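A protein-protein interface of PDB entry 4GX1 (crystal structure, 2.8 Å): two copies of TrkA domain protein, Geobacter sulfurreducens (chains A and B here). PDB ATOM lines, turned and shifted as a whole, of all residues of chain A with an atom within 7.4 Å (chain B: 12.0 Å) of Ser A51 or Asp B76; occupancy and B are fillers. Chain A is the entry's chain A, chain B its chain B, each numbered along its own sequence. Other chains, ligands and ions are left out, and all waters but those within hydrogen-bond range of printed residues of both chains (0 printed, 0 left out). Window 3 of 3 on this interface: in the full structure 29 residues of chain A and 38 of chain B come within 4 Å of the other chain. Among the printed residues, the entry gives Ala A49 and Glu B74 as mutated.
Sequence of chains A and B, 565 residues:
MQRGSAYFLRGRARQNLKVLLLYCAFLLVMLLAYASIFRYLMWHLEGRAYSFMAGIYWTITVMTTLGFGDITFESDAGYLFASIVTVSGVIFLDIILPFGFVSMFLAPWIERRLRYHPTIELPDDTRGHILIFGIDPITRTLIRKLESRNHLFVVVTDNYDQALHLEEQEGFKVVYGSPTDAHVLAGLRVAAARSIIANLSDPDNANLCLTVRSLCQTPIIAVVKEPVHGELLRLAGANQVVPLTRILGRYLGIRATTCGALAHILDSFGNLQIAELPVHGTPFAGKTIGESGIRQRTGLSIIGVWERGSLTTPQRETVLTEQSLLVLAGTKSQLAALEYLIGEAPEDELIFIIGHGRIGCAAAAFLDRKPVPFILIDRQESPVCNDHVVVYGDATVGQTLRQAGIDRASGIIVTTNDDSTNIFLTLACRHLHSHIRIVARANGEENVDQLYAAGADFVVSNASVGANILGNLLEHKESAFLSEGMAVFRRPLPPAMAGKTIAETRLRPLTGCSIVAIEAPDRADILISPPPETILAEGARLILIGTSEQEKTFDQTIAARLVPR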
ATOM      1  N   ALA A  35      22.174  22.060  21.571  1.00  0.00           N
ATOM      2  CA  ALA A  35      22.040  21.279  20.350  1.00  0.00           C
ATOM      3  C   ALA A  35      23.217  21.539  19.419  1.00  0.00           C
ATOM      4  O   ALA A  35      23.736  20.619  18.785  1.00  0.00           O
ATOM      5  CB  ALA A  35      20.724  21.600  19.652  1.00  0.00           C
ATOM      6  N   PHE A  38      26.494  20.291  20.891  1.00  0.00           N
ATOM      7  CA  PHE A  38      26.435  18.846  20.692  1.00  0.00           C
ATOM      8  C   PHE A  38      26.945  18.438  19.316  1.00  0.00           C
ATOM      9  O   PHE A  38      27.735  17.505  19.193  1.00  0.00           O
ATOM     10  CB  PHE A  38      25.006  18.328  20.863  1.00  0.00           C
ATOM     11  CG  PHE A  38      24.811  16.925  20.365  1.00  0.00           C
ATOM     12  CD1 PHE A  38      25.204  15.842  21.137  1.00  0.00           C
ATOM     13  CD2 PHE A  38      24.243  16.686  19.123  1.00  0.00           C
ATOM     14  CE1 PHE A  38      25.031  14.549  20.682  1.00  0.00           C
ATOM     15  CE2 PHE A  38      24.067  15.391  18.660  1.00  0.00           C
ATOM     16  CZ  PHE A  38      24.463  14.322  19.440  1.00  0.00           C
ATOM     17  N   ARG A  39      26.464  19.120  18.283  1.00  0.00           N
ATOM     18  CA  ARG A  39      26.877  18.826  16.924  1.00  0.00           C
ATOM     19  C   ARG A  39      28.351  19.165  16.737  1.00  0.00           C
ATOM     20  O   ARG A  39      29.106  18.398  16.130  1.00  0.00           O
ATOM     21  CB  ARG A  39      26.010  19.590  15.927  1.00  0.00           C
ATOM     22  CG  ARG A  39      24.590  19.064  15.841  1.00  0.00           C
ATOM     23  CD  ARG A  39      23.726  19.935  14.956  1.00  0.00           C
ATOM     24  NE  ARG A  39      24.201  19.979  13.578  1.00  0.00           N
ATOM     25  CZ  ARG A  39      23.771  20.851  12.673  1.00  0.00           C
ATOM     26  NH1 ARG A  39      22.865  21.756  13.007  1.00  0.00           N
ATOM     27  NH2 ARG A  39      24.246  20.827  11.438  1.00  0.00           N
ATOM     28  N   ALA A  49      28.954  13.096  12.311  1.00  0.00           N
ATOM     29  CA  ALA A  49      28.140  14.213  11.855  1.00  0.00           C
ATOM     30  C   ALA A  49      26.685  13.939  12.154  1.00  0.00           C
ATOM     31  O   ALA A  49      26.138  12.933  11.707  1.00  0.00           O
ATOM     32  CB  ALA A  49      28.336  14.452  10.381  1.00  0.00           C
ATOM     33  N   TYR A  50      26.075  14.831  12.929  1.00  0.00           N
ATOM     34  CA  TYR A  50      24.658  14.751  13.257  1.00  0.00           C
ATOM     35  C   TYR A  50      23.909  15.962  12.714  1.00  0.00           C
ATOM     36  O   TYR A  50      24.477  17.050  12.571  1.00  0.00           O
ATOM     37  CB  TYR A  50      24.455  14.644  14.773  1.00  0.00           C
ATOM     38  CG  TYR A  50      24.706  13.258  15.316  1.00  0.00           C
ATOM     39  CD1 TYR A  50      23.752  12.259  15.176  1.00  0.00           C
ATOM     40  CD2 TYR A  50      25.898  12.944  15.958  1.00  0.00           C
ATOM     41  CE1 TYR A  50      23.970  10.990  15.659  1.00  0.00           C
ATOM     42  CE2 TYR A  50      26.128  11.676  16.442  1.00  0.00           C
ATOM     43  CZ  TYR A  50      25.158  10.702  16.290  1.00  0.00           C
ATOM     44  OH  TYR A  50      25.374   9.430  16.772  1.00  0.00           O
ATOM     45  N   SER A  51      22.629  15.764  12.415  1.00  0.00           N
ATOM     46  CA  SER A  51      21.784  16.828  11.885  1.00  0.00           C
ATOM     47  C   SER A  51      21.333  17.781  12.981  1.00  0.00           C
ATOM     48  O   SER A  51      21.523  17.521  14.170  1.00  0.00           O
ATOM     49  CB  SER A  51      20.551  16.238  11.202  1.00  0.00           C
ATOM     50  OG  SER A  51      19.663  15.681  12.157  1.00  0.00           O
ATOM     51  N   PHE A  52      20.725  18.887  12.573  1.00  0.00           N
ATOM     52  CA  PHE A  52      20.176  19.834  13.527  1.00  0.00           C
ATOM     53  C   PHE A  52      19.059  19.191  14.352  1.00  0.00           C
ATOM     54  O   PHE A  52      18.997  19.357  15.574  1.00  0.00           O
ATOM     55  CB  PHE A  52      19.670  21.093  12.814  1.00  0.00           C
ATOM     56  CG  PHE A  52      19.035  22.084  13.731  1.00  0.00           C
ATOM     57  CD1 PHE A  52      17.739  22.520  13.512  1.00  0.00           C
ATOM     58  CD2 PHE A  52      19.722  22.552  14.839  1.00  0.00           C
ATOM     59  CE1 PHE A  52      17.148  23.423  14.371  1.00  0.00           C
ATOM     60  CE2 PHE A  52      19.136  23.450  15.701  1.00  0.00           C
ATOM     61  CZ  PHE A  52      17.847  23.889  15.466  1.00  0.00           C
ATOM     62  N   MET A  53      18.191  18.446  13.676  1.00  0.00           N
ATOM     63  CA  MET A  53      17.085  17.783  14.345  1.00  0.00           C
ATOM     64  C   MET A  53      17.623  16.781  15.344  1.00  0.00           C
ATOM     65  O   MET A  53      17.000  16.512  16.369  1.00  0.00           O
ATOM     66  CB  MET A  53      16.184  17.081  13.328  1.00  0.00           C
ATOM     67  CG  MET A  53      14.868  16.598  13.902  1.00  0.00           C
ATOM     68  SD  MET A  53      13.951  17.919  14.730  1.00  0.00           S
ATOM     69  CE  MET A  53      13.973  17.351  16.429  1.00  0.00           C
ATOM     70  N   ALA A  54      18.791  16.231  15.049  1.00  0.00           N
ATOM     71  CA  ALA A  54      19.370  15.221  15.918  1.00  0.00           C
ATOM     72  C   ALA A  54      19.881  15.868  17.198  1.00  0.00           C
ATOM     73  O   ALA A  54      19.860  15.253  18.260  1.00  0.00           O
ATOM     74  CB  ALA A  54      20.483  14.464  15.202  1.00  0.00           C
ATOM     75  N   GLY A  55      20.329  17.116  17.086  1.00  0.00           N
ATOM     76  CA  GLY A  55      20.839  17.857  18.227  1.00  0.00           C
ATOM     77  C   GLY A  55      19.746  18.271  19.193  1.00  0.00           C
ATOM     78  O   GLY A  55      19.926  18.213  20.408  1.00  0.00           O
ATOM     79  N   ILE A  56      18.618  18.708  18.639  1.00  0.00           N
ATOM     80  CA  ILE A  56      17.418  18.993  19.418  1.00  0.00           C
ATOM     81  C   ILE A  56      16.964  17.727  20.149  1.00  0.00           C
ATOM     82  O   ILE A  56      16.861  17.707  21.381  1.00  0.00           O
ATOM     83  CB  ILE A  56      16.262  19.473  18.507  1.00  0.00           C
ATOM     84  CG1 ILE A  56      16.706  20.652  17.640  1.00  0.00           C
ATOM     85  CG2 ILE A  56      15.042  19.839  19.330  1.00  0.00           C
ATOM     86  CD1 ILE A  56      17.110  21.875  18.422  1.00  0.00           C
ATOM     87  N   TYR A  57      16.703  16.680  19.368  1.00  0.00           N
ATOM     88  CA  TYR A  57      16.267  15.382  19.877  1.00  0.00           C
ATOM     89  C   TYR A  57      17.179  14.858  20.978  1.00  0.00           C
ATOM     90  O   TYR A  57      16.700  14.378  22.000  1.00  0.00           O
ATOM     91  CB  TYR A  57      16.169  14.389  18.716  1.00  0.00           C
ATOM     92  CG  TYR A  57      16.127  12.914  19.083  1.00  0.00           C
ATOM     93  CD1 TYR A  57      14.946  12.307  19.504  1.00  0.00           C
ATOM     94  CD2 TYR A  57      17.262  12.117  18.953  1.00  0.00           C
ATOM     95  CE1 TYR A  57      14.909  10.957  19.816  1.00  0.00           C
ATOM     96  CE2 TYR A  57      17.236  10.768  19.261  1.00  0.00           C
ATOM     97  CZ  TYR A  57      16.059  10.188  19.691  1.00  0.00           C
ATOM     98  OH  TYR A  57      16.037   8.840  19.988  1.00  0.00           O
ATOM     99  N   ILE B  37       0.143   6.652  15.818  1.00  0.00           N
ATOM    100  CA  ILE B  37       1.045   7.425  14.975  1.00  0.00           C
ATOM    101  C   ILE B  37       2.459   6.837  14.992  1.00  0.00           C
ATOM    102  O   ILE B  37       3.157   6.861  13.976  1.00  0.00           O
ATOM    103  CB  ILE B  37       1.080   8.908  15.391  1.00  0.00           C
ATOM    104  CG1 ILE B  37      -0.323   9.508  15.316  1.00  0.00           C
ATOM    105  CG2 ILE B  37       2.037   9.694  14.506  1.00  0.00           C
ATOM    106  CD1 ILE B  37      -0.434  10.862  15.980  1.00  0.00           C
ATOM    107  N   LEU B  41       4.442   5.917  11.599  1.00  0.00           N
ATOM    108  CA  LEU B  41       5.708   6.537  11.216  1.00  0.00           C
ATOM    109  C   LEU B  41       6.833   5.518  11.091  1.00  0.00           C
ATOM    110  O   LEU B  41       7.649   5.614  10.181  1.00  0.00           O
ATOM    111  CB  LEU B  41       6.106   7.642  12.196  1.00  0.00           C
ATOM    112  CG  LEU B  41       5.141   8.823  12.332  1.00  0.00           C
ATOM    113  CD1 LEU B  41       5.655   9.842  13.341  1.00  0.00           C
ATOM    114  CD2 LEU B  41       4.882   9.477  10.984  1.00  0.00           C
ATOM    115  N   MET B  42       6.883   4.548  12.002  1.00  0.00           N
ATOM    116  CA  MET B  42       7.889   3.492  11.909  1.00  0.00           C
ATOM    117  C   MET B  42       7.768   2.793  10.566  1.00  0.00           C
ATOM    118  O   MET B  42       8.770   2.446   9.934  1.00  0.00           O
ATOM    119  CB  MET B  42       7.745   2.475  13.039  1.00  0.00           C
ATOM    120  CG  MET B  42       8.485   2.855  14.302  1.00  0.00           C
ATOM    121  SD  MET B  42      10.239   3.092  13.997  1.00  0.00           S
ATOM    122  CE  MET B  42      10.865   3.440  15.639  1.00  0.00           C
ATOM    123  N   HIS B  44       6.110   4.058   7.551  1.00  0.00           N
ATOM    124  CA  HIS B  44       6.310   4.882   6.364  1.00  0.00           C
ATOM    125  C   HIS B  44       7.659   5.598   6.305  1.00  0.00           C
ATOM    126  O   HIS B  44       8.128   5.962   5.224  1.00  0.00           O
ATOM    127  CB  HIS B  44       5.159   5.869   6.195  1.00  0.00           C
ATOM    128  CG  HIS B  44       3.880   5.226   5.765  1.00  0.00           C
ATOM    129  ND1 HIS B  44       2.862   4.928   6.645  1.00  0.00           N
ATOM    130  CD2 HIS B  44       3.460   4.809   4.548  1.00  0.00           C
ATOM    131  CE1 HIS B  44       1.865   4.363   5.988  1.00  0.00           C
ATOM    132  NE2 HIS B  44       2.202   4.282   4.714  1.00  0.00           N
ATOM    133  N   LEU B  45       8.289   5.788   7.455  1.00  0.00           N
ATOM    134  CA  LEU B  45       9.550   6.520   7.497  1.00  0.00           C
ATOM    135  C   LEU B  45      10.780   5.618   7.542  1.00  0.00           C
ATOM    136  O   LEU B  45      11.866   6.038   7.150  1.00  0.00           O
ATOM    137  CB  LEU B  45       9.571   7.495   8.682  1.00  0.00           C
ATOM    138  CG  LEU B  45       8.612   8.687   8.626  1.00  0.00           C
ATOM    139  CD1 LEU B  45       8.483   9.344   9.993  1.00  0.00           C
ATOM    140  CD2 LEU B  45       9.085   9.694   7.588  1.00  0.00           C
ATOM    141  N   GLU B  46      10.622   4.393   8.039  1.00  0.00           N
ATOM    142  CA  GLU B  46      11.774   3.518   8.258  1.00  0.00           C
ATOM    143  C   GLU B  46      11.545   2.086   7.774  1.00  0.00           C
ATOM    144  O   GLU B  46      12.465   1.270   7.767  1.00  0.00           O
ATOM    145  CB  GLU B  46      12.187   3.519   9.738  1.00  0.00           C
ATOM    146  CG  GLU B  46      12.145   4.900  10.400  1.00  0.00           C
ATOM    147  CD  GLU B  46      13.375   5.215  11.230  1.00  0.00           C
ATOM    148  OE1 GLU B  46      13.510   6.384  11.662  1.00  0.00           O
ATOM    149  OE2 GLU B  46      14.202   4.300  11.448  1.00  0.00           O
ATOM    150  N   GLY B  47      10.323   1.780   7.362  1.00  0.00           N
ATOM    151  CA  GLY B  47      10.015   0.453   6.868  1.00  0.00           C
ATOM    152  C   GLY B  47      10.117  -0.596   7.952  1.00  0.00           C
ATOM    153  O   GLY B  47      10.547  -1.721   7.702  1.00  0.00           O
ATOM    154  N   ARG B  48       9.731  -0.219   9.165  1.00  0.00           N
ATOM    155  CA  ARG B  48       9.674  -1.155  10.280  1.00  0.00           C
ATOM    156  C   ARG B  48       8.233  -1.371  10.713  1.00  0.00           C
ATOM    157  O   ARG B  48       7.460  -0.424  10.805  1.00  0.00           O
ATOM    158  CB  ARG B  48      10.457  -0.627  11.470  1.00  0.00           C
ATOM    159  CG  ARG B  48      11.892  -0.289  11.209  1.00  0.00           C
ATOM    160  CD  ARG B  48      12.601  -0.241  12.538  1.00  0.00           C
ATOM    161  NE  ARG B  48      13.238   1.042  12.776  1.00  0.00           N
ATOM    162  CZ  ARG B  48      13.632   1.473  13.970  1.00  0.00           C
ATOM    163  NH1 ARG B  48      13.435   0.732  15.054  1.00  0.00           N
ATOM    164  NH2 ARG B  48      14.210   2.661  14.079  1.00  0.00           N
ATOM    165  N   TRP B  58       6.072   1.561  23.678  1.00  0.00           N
ATOM    166  CA  TRP B  58       7.018   2.614  23.336  1.00  0.00           C
ATOM    167  C   TRP B  58       6.540   3.964  23.866  1.00  0.00           C
ATOM    168  O   TRP B  58       7.311   4.730  24.451  1.00  0.00           O
ATOM    169  CB  TRP B  58       7.219   2.683  21.818  1.00  0.00           C
ATOM    170  CG  TRP B  58       8.119   3.812  21.375  1.00  0.00           C
ATOM    171  CD1 TRP B  58       9.476   3.772  21.236  1.00  0.00           C
ATOM    172  CD2 TRP B  58       7.720   5.144  21.016  1.00  0.00           C
ATOM    173  NE1 TRP B  58       9.944   4.993  20.816  1.00  0.00           N
ATOM    174  CE2 TRP B  58       8.887   5.851  20.669  1.00  0.00           C
ATOM    175  CE3 TRP B  58       6.487   5.808  20.955  1.00  0.00           C
ATOM    176  CZ2 TRP B  58       8.861   7.181  20.267  1.00  0.00           C
ATOM    177  CZ3 TRP B  58       6.462   7.127  20.554  1.00  0.00           C
ATOM    178  CH2 TRP B  58       7.642   7.800  20.215  1.00  0.00           C
ATOM    179  N   THR B  72      14.047   2.950  18.901  1.00  0.00           N
ATOM    180  CA  THR B  72      14.249   4.364  18.594  1.00  0.00           C
ATOM    181  C   THR B  72      14.142   4.607  17.089  1.00  0.00           C
ATOM    182  O   THR B  72      14.228   3.677  16.298  1.00  0.00           O
ATOM    183  CB  THR B  72      15.624   4.885  19.075  1.00  0.00           C
ATOM    184  OG1 THR B  72      16.657   4.336  18.255  1.00  0.00           O
ATOM    185  CG2 THR B  72      15.890   4.513  20.518  1.00  0.00           C
ATOM    186  N   PHE B  73      13.942   5.860  16.704  1.00  0.00           N
ATOM    187  CA  PHE B  73      13.907   6.216  15.299  1.00  0.00           C
ATOM    188  C   PHE B  73      15.329   6.500  14.811  1.00  0.00           C
ATOM    189  O   PHE B  73      16.261   6.635  15.603  1.00  0.00           O
ATOM    190  CB  PHE B  73      13.021   7.442  15.080  1.00  0.00           C
ATOM    191  CG  PHE B  73      11.553   7.174  15.251  1.00  0.00           C
ATOM    192  CD1 PHE B  73      10.752   6.891  14.155  1.00  0.00           C
ATOM    193  CD2 PHE B  73      10.968   7.215  16.502  1.00  0.00           C
ATOM    194  CE1 PHE B  73       9.394   6.653  14.303  1.00  0.00           C
ATOM    195  CE2 PHE B  73       9.612   6.967  16.651  1.00  0.00           C
ATOM    196  CZ  PHE B  73       8.829   6.685  15.547  1.00  0.00           C
ATOM    197  N   GLU B  74      15.494   6.579  13.498  1.00  0.00           N
ATOM    198  CA  GLU B  74      16.779   6.919  12.906  1.00  0.00           C
ATOM    199  C   GLU B  74      16.635   8.138  12.005  1.00  0.00           C
ATOM    200  O   GLU B  74      17.609   8.826  11.717  1.00  0.00           O
ATOM    201  CB  GLU B  74      17.339   5.735  12.122  1.00  0.00           C
ATOM    202  CG  GLU B  74      18.167   4.745  12.952  1.00  0.00           C
ATOM    203  CD  GLU B  74      18.895   3.743  12.054  1.00  0.00           C
ATOM    204  OE1 GLU B  74      18.266   3.209  11.105  1.00  0.00           O
ATOM    205  OE2 GLU B  74      20.089   3.476  12.300  1.00  0.00           O
ATOM    206  N   SER B  75      15.410   8.391  11.559  1.00  0.00           N
ATOM    207  CA  SER B  75      15.121   9.536  10.700  1.00  0.00           C
ATOM    208  C   SER B  75      14.953  10.805  11.517  1.00  0.00           C
ATOM    209  O   SER B  75      14.685  10.750  12.716  1.00  0.00           O
ATOM    210  CB  SER B  75      13.846   9.289   9.895  1.00  0.00           C
ATOM    211  OG  SER B  75      12.708   9.264  10.741  1.00  0.00           O
ATOM    212  N   ASP B  76      15.099  11.951  10.867  1.00  0.00           N
ATOM    213  CA  ASP B  76      14.896  13.229  11.535  1.00  0.00           C
ATOM    214  C   ASP B  76      13.429  13.433  11.902  1.00  0.00           C
ATOM    215  O   ASP B  76      13.118  13.960  12.970  1.00  0.00           O
ATOM    216  CB  ASP B  76      15.390  14.373  10.651  1.00  0.00           C
ATOM    217  CG  ASP B  76      16.894  14.552  10.720  1.00  0.00           C
ATOM    218  OD1 ASP B  76      17.567  13.721  11.372  1.00  0.00           O
ATOM    219  OD2 ASP B  76      17.401  15.526  10.123  1.00  0.00           O
ATOM    220  N   ALA B  77      12.531  13.013  11.016  1.00  0.00           N
ATOM    221  CA  ALA B  77      11.100  13.142  11.261  1.00  0.00           C
ATOM    222  C   ALA B  77      10.696  12.244  12.416  1.00  0.00           C
ATOM    223  O   ALA B  77       9.750  12.532  13.148  1.00  0.00           O
ATOM    224  CB  ALA B  77      10.319  12.791  10.023  1.00  0.00           C
ATOM    225  N   GLY B  78      11.419  11.144  12.569  1.00  0.00           N
ATOM    226  CA  GLY B  78      11.217  10.270  13.703  1.00  0.00           C
ATOM    227  C   GLY B  78      11.753  10.909  14.964  1.00  0.00           C
ATOM    228  O   GLY B  78      11.213  10.709  16.044  1.00  0.00           O
ATOM    229  N   TYR B  79      12.823  11.681  14.827  1.00  0.00           N
ATOM    230  CA  TYR B  79      13.384  12.407  15.957  1.00  0.00           C
ATOM    231  C   TYR B  79      12.429  13.497  16.440  1.00  0.00           C
ATOM    232  O   TYR B  79      12.204  13.650  17.640  1.00  0.00           O
ATOM    233  CB  TYR B  79      14.721  13.034  15.570  1.00  0.00           C
ATOM    234  CG  TYR B  79      15.840  12.046  15.421  1.00  0.00           C
ATOM    235  CD1 TYR B  79      16.942  12.338  14.626  1.00  0.00           C
ATOM    236  CD2 TYR B  79      15.800  10.818  16.075  1.00  0.00           C
ATOM    237  CE1 TYR B  79      17.981  11.430  14.482  1.00  0.00           C
ATOM    238  CE2 TYR B  79      16.833   9.907  15.941  1.00  0.00           C
ATOM    239  CZ  TYR B  79      17.921  10.221  15.140  1.00  0.00           C
ATOM    240  OH  TYR B  79      18.955   9.330  14.998  1.00  0.00           O
ATOM    241  N   LEU B  80      11.887  14.251  15.486  1.00  0.00           N
ATOM    242  CA  LEU B  80      10.924  15.307  15.760  1.00  0.00           C
ATOM    243  C   LEU B  80       9.728  14.731  16.502  1.00  0.00           C
ATOM    244  O   LEU B  80       9.239  15.325  17.463  1.00  0.00           O
ATOM    245  CB  LEU B  80      10.465  15.951  14.449  1.00  0.00           C
ATOM    246  CG  LEU B  80       9.826  17.351  14.412  1.00  0.00           C
ATOM    247  CD1 LEU B  80       8.438  17.293  13.773  1.00  0.00           C
ATOM    248  CD2 LEU B  80       9.779  18.037  15.783  1.00  0.00           C
ATOM    249  N   PHE B  81       9.268  13.562  16.067  1.00  0.00           N
ATOM    250  CA  PHE B  81       8.126  12.923  16.709  1.00  0.00           C
ATOM    251  C   PHE B  81       8.453  12.407  18.105  1.00  0.00           C
ATOM    252  O   PHE B  81       7.656  12.577  19.027  1.00  0.00           O
ATOM    253  CB  PHE B  81       7.569  11.789  15.854  1.00  0.00           C
ATOM    254  CG  PHE B  81       6.405  11.076  16.484  1.00  0.00           C
ATOM    255  CD1 PHE B  81       5.147  11.662  16.511  1.00  0.00           C
ATOM    256  CD2 PHE B  81       6.563   9.813  17.038  1.00  0.00           C
ATOM    257  CE1 PHE B  81       4.071  11.005  17.081  1.00  0.00           C
ATOM    258  CE2 PHE B  81       5.492   9.149  17.609  1.00  0.00           C
ATOM    259  CZ  PHE B  81       4.243   9.747  17.631  1.00  0.00           C
ATOM    260  N   ALA B  82       9.613  11.774  18.259  1.00  0.00           N
ATOM    261  CA  ALA B  82      10.014  11.255  19.562  1.00  0.00           C
ATOM    262  C   ALA B  82      10.081  12.412  20.541  1.00  0.00           C
ATOM    263  O   ALA B  82       9.644  12.302  21.685  1.00  0.00           O
ATOM    264  CB  ALA B  82      11.354  10.543  19.486  1.00  0.00           C
ATOM    265  N   SER B  83      10.615  13.529  20.066  1.00  0.00           N
ATOM    266  CA  SER B  83      10.733  14.732  20.874  1.00  0.00           C
ATOM    267  C   SER B  83       9.365  15.260  21.306  1.00  0.00           C
ATOM    268  O   SER B  83       9.159  15.576  22.478  1.00  0.00           O
ATOM    269  CB  SER B  83      11.499  15.804  20.103  1.00  0.00           C
ATOM    270  OG  SER B  83      12.769  15.314  19.719  1.00  0.00           O
ATOM    271  N   ILE B  84       8.439  15.352  20.355  1.00  0.00           N
ATOM    272  CA  ILE B  84       7.096  15.831  20.645  1.00  0.00           C
ATOM    273  C   ILE B  84       6.437  14.974  21.720  1.00  0.00           C
ATOM    274  O   ILE B  84       5.900  15.496  22.696  1.00  0.00           O
ATOM    275  CB  ILE B  84       6.221  15.859  19.382  1.00  0.00           C
ATOM    276  CG1 ILE B  84       6.615  17.037  18.492  1.00  0.00           C
ATOM    277  CG2 ILE B  84       4.757  15.973  19.751  1.00  0.00           C
ATOM    278  CD1 ILE B  84       5.871  17.080  17.179  1.00  0.00           C
ATOM    279  N   VAL B  85       6.502  13.659  21.555  1.00  0.00           N
ATOM    280  CA  VAL B  85       5.933  12.750  22.539  1.00  0.00           C
ATOM    281  C   VAL B  85       6.623  12.925  23.887  1.00  0.00           C
ATOM    282  O   VAL B  85       5.989  12.850  24.937  1.00  0.00           O
ATOM    283  CB  VAL B  85       6.037  11.282  22.080  1.00  0.00           C
ATOM    284  CG1 VAL B  85       5.550  10.336  23.171  1.00  0.00           C
ATOM    285  CG2 VAL B  85       5.236  11.076  20.807  1.00  0.00           C
ATOM    286  N   THR B  86       7.922  13.187  23.853  1.00  0.00           N
ATOM    287  CA  THR B  86       8.695  13.308  25.079  1.00  0.00           C
ATOM    288  C   THR B  86       8.269  14.526  25.887  1.00  0.00           C
ATOM    289  O   THR B  86       8.058  14.440  27.098  1.00  0.00           O
ATOM    290  CB  THR B  86      10.197  13.392  24.785  1.00  0.00           C
ATOM    291  OG1 THR B  86      10.630  12.188  24.140  1.00  0.00           O
ATOM    292  CG2 THR B  86      10.956  13.550  26.057  1.00  0.00           C
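CG of Met A53 touches O of Asp B76, 3.3 Å away.
Met A53 touches Tyr B79.
Leu B80 touches Met A53 (CA to CE, 3.7 Å).
Ala A54 touches Tyr B79.
Tyr B79 touches Tyr A57.
CE1 of Tyr A57 touches CB of Ala B82, at 3.6 Å.
Ser B83 touches Tyr A57 (OG to CA, 3.5 Å).
No residue of chain B comes within 4 Å of Arg A39.
No residue of chain B comes within 4 Å of Phe A52.
Of the printed residues of chain B, Ala A54 touches Tyr B79 (3.98 Å).
No residue of chain B comes within 4 Å of Gly A55.
Asp B76 touches just these residues of chain A: Ser A51 and Met A53.
Of the printed residues of chain A, Tyr B79 touches Met A53 (3.9 Å), Ala A54 (3.98 Å) and Tyr A57 (3.5 Å).
Of the printed residues of chain A, Leu B80 touches Met A53.
Of the printed residues of chain A, Ser B83 touches Tyr A57.
Printed residues of chain A that touch a printed residue of chain B: Ser A51, Met A53, Ala A54 and Tyr A57.
Hydrophobic or aromatic side chains of chain A that line the printed part of chain B: Met A53, Ala A54 and Tyr A57.
Along chain A the printed residues that touch a printed residue of chain B span positions 51 to 57.
Hydrophobic or aromatic side chains of chain B that line the printed part of chain A: Tyr B79 and Ala B82.
Along chain B the printed residues that touch a printed residue of chain A span positions 76 to 83.
The side-chain hydroxyl (OG) of Ser A51 lies within hydrogen-bond range of the side-chain carboxylate (OD1) of Asp B76 (3.0 Å).
No position is printed for both chains.
O of Ala B82 lies within hydrogen-bond range of OG1 of Thr B86 (2.6 Å).
The backbone NH (N) of Ala A54 sits at hydrogen-bond distance from the side-chain hydroxyl (OG) of Ser A51, 3.1 Å away.
The backbone NH (N) of Met A53 sits close to the side-chain hydroxyl (OG) of Ser A51 (3.5 Å).
OG of Ser B83 is in hydrogen-bond range of O of Tyr B79 (2.7 Å).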
